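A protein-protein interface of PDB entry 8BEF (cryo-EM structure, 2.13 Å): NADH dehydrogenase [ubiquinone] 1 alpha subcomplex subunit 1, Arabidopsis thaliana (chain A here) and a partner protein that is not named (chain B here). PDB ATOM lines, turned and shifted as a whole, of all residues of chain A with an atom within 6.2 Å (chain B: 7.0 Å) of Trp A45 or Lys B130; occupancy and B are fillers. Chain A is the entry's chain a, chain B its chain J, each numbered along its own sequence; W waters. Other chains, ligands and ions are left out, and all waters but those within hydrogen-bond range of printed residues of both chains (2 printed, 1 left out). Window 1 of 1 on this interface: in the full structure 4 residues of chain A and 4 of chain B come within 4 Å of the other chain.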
ATOM      1  N   ASP A  43     -18.191  -8.381  18.238  1.00  0.00           N
ATOM      2  CA  ASP A  43     -19.535  -8.503  18.781  1.00  0.00           C
ATOM      3  C   ASP A  43     -20.002  -7.169  19.373  1.00  0.00           C
ATOM      4  O   ASP A  43     -19.341  -6.134  19.227  1.00  0.00           O
ATOM      5  CB  ASP A  43     -19.588  -9.643  19.805  1.00  0.00           C
ATOM      6  CG  ASP A  43     -18.632  -9.446  20.975  1.00  0.00           C
ATOM      7  OD1 ASP A  43     -18.003  -8.374  21.086  1.00  0.00           O
ATOM      8  OD2 ASP A  43     -18.515 -10.378  21.795  1.00  0.00           O
ATOM      9  N   GLU A  44     -21.165  -7.202  20.031  1.00  0.00           N
ATOM     10  CA  GLU A  44     -21.730  -6.000  20.640  1.00  0.00           C
ATOM     11  C   GLU A  44     -20.747  -5.351  21.607  1.00  0.00           C
ATOM     12  O   GLU A  44     -20.620  -4.120  21.646  1.00  0.00           O
ATOM     13  CB  GLU A  44     -23.026  -6.346  21.376  1.00  0.00           C
ATOM     14  CG  GLU A  44     -24.247  -6.487  20.496  1.00  0.00           C
ATOM     15  CD  GLU A  44     -24.177  -7.691  19.579  1.00  0.00           C
ATOM     16  OE1 GLU A  44     -23.567  -8.710  19.965  1.00  0.00           O
ATOM     17  OE2 GLU A  44     -24.747  -7.623  18.476  1.00  0.00           O
ATOM     18  N   TRP A  45     -20.049  -6.168  22.397  1.00  0.00           N
ATOM     19  CA  TRP A  45     -19.097  -5.643  23.369  1.00  0.00           C
ATOM     20  C   TRP A  45     -17.976  -4.869  22.684  1.00  0.00           C
ATOM     21  O   TRP A  45     -17.606  -3.778  23.126  1.00  0.00           O
ATOM     22  CB  TRP A  45     -18.527  -6.787  24.208  1.00  0.00           C
ATOM     23  CG  TRP A  45     -17.527  -6.343  25.230  1.00  0.00           C
ATOM     24  CD1 TRP A  45     -16.190  -6.161  25.042  1.00  0.00           C
ATOM     25  CD2 TRP A  45     -17.787  -6.024  26.601  1.00  0.00           C
ATOM     26  NE1 TRP A  45     -15.599  -5.749  26.212  1.00  0.00           N
ATOM     27  CE2 TRP A  45     -16.558  -5.657  27.184  1.00  0.00           C
ATOM     28  CE3 TRP A  45     -18.939  -6.014  27.394  1.00  0.00           C
ATOM     29  CZ2 TRP A  45     -16.449  -5.284  28.523  1.00  0.00           C
ATOM     30  CZ3 TRP A  45     -18.829  -5.644  28.720  1.00  0.00           C
ATOM     31  CH2 TRP A  45     -17.593  -5.283  29.271  1.00  0.00           C
ATOM     32  N   ASP A  46     -17.420  -5.423  21.606  1.00  0.00           N
ATOM     33  CA  ASP A  46     -16.318  -4.754  20.919  1.00  0.00           C
ATOM     34  C   ASP A  46     -16.769  -3.440  20.292  1.00  0.00           C
ATOM     35  O   ASP A  46     -16.041  -2.442  20.333  1.00  0.00           O
ATOM     36  CB  ASP A  46     -15.718  -5.684  19.865  1.00  0.00           C
ATOM     37  CG  ASP A  46     -15.108  -6.934  20.470  1.00  0.00           C
ATOM     38  OD1 ASP A  46     -14.392  -6.822  21.484  1.00  0.00           O
ATOM     39  OD2 ASP A  46     -15.349  -8.034  19.935  1.00  0.00           O
ATOM     40  N   VAL A  47     -17.970  -3.422  19.709  1.00  0.00           N
ATOM     41  CA  VAL A  47     -18.502  -2.199  19.114  1.00  0.00           C
ATOM     42  C   VAL A  47     -18.714  -1.129  20.181  1.00  0.00           C
ATOM     43  O   VAL A  47     -18.368   0.045  19.985  1.00  0.00           O
ATOM     44  CB  VAL A  47     -19.801  -2.509  18.344  1.00  0.00           C
ATOM     45  CG1 VAL A  47     -20.438  -1.240  17.839  1.00  0.00           C
ATOM     46  CG2 VAL A  47     -19.515  -3.449  17.183  1.00  0.00           C
ATOM     47  N   ALA A  48     -19.290  -1.515  21.325  1.00  0.00           N
ATOM     48  CA  ALA A  48     -19.463  -0.565  22.420  1.00  0.00           C
ATOM     49  C   ALA A  48     -18.118  -0.064  22.936  1.00  0.00           C
ATOM     50  O   ALA A  48     -17.975   1.118  23.271  1.00  0.00           O
ATOM     51  CB  ALA A  48     -20.271  -1.204  23.551  1.00  0.00           C
ATOM     52  N   MET A  49     -17.120  -0.950  23.001  1.00  0.00           N
ATOM     53  CA  MET A  49     -15.781  -0.547  23.416  1.00  0.00           C
ATOM     54  C   MET A  49     -15.193   0.490  22.471  1.00  0.00           C
ATOM     55  O   MET A  49     -14.628   1.492  22.915  1.00  0.00           O
ATOM     56  CB  MET A  49     -14.865  -1.769  23.506  1.00  0.00           C
ATOM     57  CG  MET A  49     -15.016  -2.708  24.722  1.00  0.00           C
ATOM     58  SD  MET A  49     -15.335  -2.028  26.375  1.00  0.00           S
ATOM     59  CE  MET A  49     -17.059  -1.552  26.323  1.00  0.00           C
ATOM     60  N   GLU A  50     -15.307   0.263  21.162  1.00  0.00           N
ATOM     61  CA  GLU A  50     -14.773   1.224  20.199  1.00  0.00           C
ATOM     62  C   GLU A  50     -15.500   2.564  20.275  1.00  0.00           C
ATOM     63  O   GLU A  50     -14.863   3.628  20.246  1.00  0.00           O
ATOM     64  CB  GLU A  50     -14.836   0.641  18.787  1.00  0.00           C
ATOM     65  CG  GLU A  50     -13.907  -0.548  18.572  1.00  0.00           C
ATOM     66  CD  GLU A  50     -14.025  -1.171  17.193  1.00  0.00           C
ATOM     67  OE1 GLU A  50     -14.966  -0.799  16.456  1.00  0.00           O
ATOM     68  OE2 GLU A  50     -13.207  -2.049  16.854  1.00  0.00           O
ATOM     69  N   THR B 125     -26.765   2.676  27.977  1.00  0.00           N
ATOM     70  CA  THR B 125     -26.098   1.425  27.637  1.00  0.00           C
ATOM     71  C   THR B 125     -25.910   0.586  28.893  1.00  0.00           C
ATOM     72  O   THR B 125     -25.326   1.054  29.875  1.00  0.00           O
ATOM     73  CB  THR B 125     -24.748   1.688  26.970  1.00  0.00           C
ATOM     74  OG1 THR B 125     -24.960   2.271  25.679  1.00  0.00           O
ATOM     75  CG2 THR B 125     -23.964   0.398  26.819  1.00  0.00           C
ATOM     76  N   VAL B 126     -26.401  -0.648  28.855  1.00  0.00           N
ATOM     77  CA  VAL B 126     -26.186  -1.629  29.913  1.00  0.00           C
ATOM     78  C   VAL B 126     -25.192  -2.650  29.380  1.00  0.00           C
ATOM     79  O   VAL B 126     -25.526  -3.454  28.502  1.00  0.00           O
ATOM     80  CB  VAL B 126     -27.496  -2.303  30.345  1.00  0.00           C
ATOM     81  CG1 VAL B 126     -27.246  -3.252  31.513  1.00  0.00           C
ATOM     82  CG2 VAL B 126     -28.539  -1.260  30.698  1.00  0.00           C
ATOM     83  N   TYR B 127     -23.966  -2.625  29.906  1.00  0.00           N
ATOM     84  CA  TYR B 127     -22.944  -3.533  29.408  1.00  0.00           C
ATOM     85  C   TYR B 127     -23.146  -4.963  29.899  1.00  0.00           C
ATOM     86  O   TYR B 127     -22.544  -5.883  29.338  1.00  0.00           O
ATOM     87  CB  TYR B 127     -21.549  -3.047  29.809  1.00  0.00           C
ATOM     88  CG  TYR B 127     -21.114  -1.730  29.209  1.00  0.00           C
ATOM     89  CD1 TYR B 127     -20.573  -1.673  27.936  1.00  0.00           C
ATOM     90  CD2 TYR B 127     -21.210  -0.546  29.934  1.00  0.00           C
ATOM     91  CE1 TYR B 127     -20.165  -0.476  27.385  1.00  0.00           C
ATOM     92  CE2 TYR B 127     -20.802   0.657  29.394  1.00  0.00           C
ATOM     93  CZ  TYR B 127     -20.277   0.685  28.115  1.00  0.00           C
ATOM     94  OH  TYR B 127     -19.866   1.872  27.559  1.00  0.00           O
ATOM     95  N   ALA B 128     -23.982  -5.168  30.920  1.00  0.00           N
ATOM     96  CA  ALA B 128     -24.140  -6.502  31.495  1.00  0.00           C
ATOM     97  C   ALA B 128     -24.676  -7.491  30.466  1.00  0.00           C
ATOM     98  O   ALA B 128     -24.212  -8.635  30.393  1.00  0.00           O
ATOM     99  CB  ALA B 128     -25.057  -6.445  32.715  1.00  0.00           C
ATOM    100  N   GLY B 129     -25.645  -7.070  29.658  1.00  0.00           N
ATOM    101  CA  GLY B 129     -26.173  -7.936  28.620  1.00  0.00           C
ATOM    102  C   GLY B 129     -25.255  -8.132  27.432  1.00  0.00           C
ATOM    103  O   GLY B 129     -25.583  -8.932  26.549  1.00  0.00           O
ATOM    104  N   LYS B 130     -24.120  -7.437  27.391  1.00  0.00           N
ATOM    105  CA  LYS B 130     -23.197  -7.493  26.265  1.00  0.00           C
ATOM    106  C   LYS B 130     -21.980  -8.377  26.515  1.00  0.00           C
ATOM    107  O   LYS B 130     -21.138  -8.508  25.622  1.00  0.00           O
ATOM    108  CB  LYS B 130     -22.727  -6.081  25.897  1.00  0.00           C
ATOM    109  CG  LYS B 130     -23.716  -5.272  25.086  1.00  0.00           C
ATOM    110  CD  LYS B 130     -23.327  -3.806  25.049  1.00  0.00           C
ATOM    111  CE  LYS B 130     -24.501  -2.931  24.661  1.00  0.00           C
ATOM    112  NZ  LYS B 130     -24.359  -2.406  23.281  1.00  0.00           N
ATOM    113  N   VAL B 131     -21.856  -8.968  27.706  1.00  0.00           N
ATOM    114  CA  VAL B 131     -20.706  -9.820  27.999  1.00  0.00           C
ATOM    115  C   VAL B 131     -20.738 -11.071  27.130  1.00  0.00           C
ATOM    116  O   VAL B 131     -19.721 -11.477  26.562  1.00  0.00           O
ATOM    117  CB  VAL B 131     -20.676 -10.170  29.501  1.00  0.00           C
ATOM    118  CG1 VAL B 131     -19.715 -11.318  29.774  1.00  0.00           C
ATOM    119  CG2 VAL B 131     -20.330  -8.943  30.343  1.00  0.00           C
ATOM    120  N   ARG B 132     -21.909 -11.690  27.010  1.00  0.00           N
ATOM    121  CA  ARG B 132     -22.133 -12.901  26.211  1.00  0.00           C
ATOM    122  C   ARG B 132     -23.416 -12.710  25.416  1.00  0.00           C
ATOM    123  O   ARG B 132     -24.495 -13.088  25.876  1.00  0.00           O
ATOM    124  CB  ARG B 132     -22.213 -14.139  27.091  1.00  0.00           C
ATOM    125  CG  ARG B 132     -22.421 -15.438  26.328  1.00  0.00           C
ATOM    126  CD  ARG B 132     -22.421 -16.631  27.231  1.00  0.00           C
ATOM    127  NE  ARG B 132     -22.594 -17.897  26.532  1.00  0.00           N
ATOM    128  CZ  ARG B 132     -22.437 -19.085  27.095  1.00  0.00           C
ATOM    129  NH1 ARG B 132     -22.092 -19.202  28.368  1.00  0.00           N
ATOM    130  NH2 ARG B 132     -22.646 -20.180  26.370  1.00  0.00           N
ATOM    131  N   SER B 133     -23.287 -12.157  24.215  1.00  0.00           N
ATOM    132  CA  SER B 133     -24.449 -11.924  23.374  1.00  0.00           C
ATOM    133  C   SER B 133     -24.848 -13.205  22.653  1.00  0.00           C
ATOM    134  O   SER B 133     -23.997 -14.010  22.269  1.00  0.00           O
ATOM    135  CB  SER B 133     -24.168 -10.812  22.362  1.00  0.00           C
ATOM    136  OG  SER B 133     -22.891 -10.980  21.768  1.00  0.00           O
HETATM  137  O   HOH W   1     -21.039  -9.235  22.861  1.00  0.00           O
HETATM  138  O   HOH W   2     -19.971   2.087  24.639  1.00  0.00           O
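The side-chain carboxylate (OE1) of Glu A44 sits at hydrogen-bond distance from the side-chain hydroxyl (OG) of Ser B133 (3.0 Å).
Among the printed residues, merely in contact across the chains: Trp A45 with Lys B130 (3.4 Å), Met A49 with Tyr B127 (3.5 Å), Trp A45 with Tyr B127 (3.8 Å), Ala A48 with Tyr B127 (3.9 Å), Glu A44 with Lys B130 (3.9 Å) and Trp A45 with Val B131 (3.97 Å).
OD1 of Asp A43 sits close to N of Trp A45 (3.3 Å).
SD of Met A49 lies close to NE1 of Trp A45, at 3.7 Å.
Of the printed residues of chain B, Trp A45 touches Tyr B127, Lys B130 and Val B131.
Printed residues of chain A within 4 Å of Lys B130: Glu A44 (3.9 Å) and Trp A45 (3.4 Å).
Printed residues of chain A within 4 Å of Tyr B127: Trp A45 (3.8 Å), Ala A48 (3.9 Å) and Met A49 (3.5 Å).
Printed residues of chain B within 4 Å of Glu A44: Lys B130 (3.9 Å) and Ser B133 (3.0 Å).
The nearest printed residue of chain B that does not touch Met A49 is Lys B130 (6.8 Å).
Water W2 bridges the backbone carbonyl oxygen of Ala A48 (2.6 Å) and the side-chain hydroxyl of Tyr B127 (2.9 Å).
Water W1 lies within hydrogen-bond range of the side-chain hydroxyl of Ser B133, the backbone carbonyl oxygen of Lys B130, the side-chain carboxylate of Asp A43, the backbone NH of Trp A45 and the backbone NH of Glu A44.
Printed residues of chain A that touch a printed residue of chain B: Glu A44, Trp A45, Ala A48 and Met A49.
Hydrophobic or aromatic side chains of chain A within 4 Å of the printed part of chain B: Trp A45, Ala A48 and Met A49.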
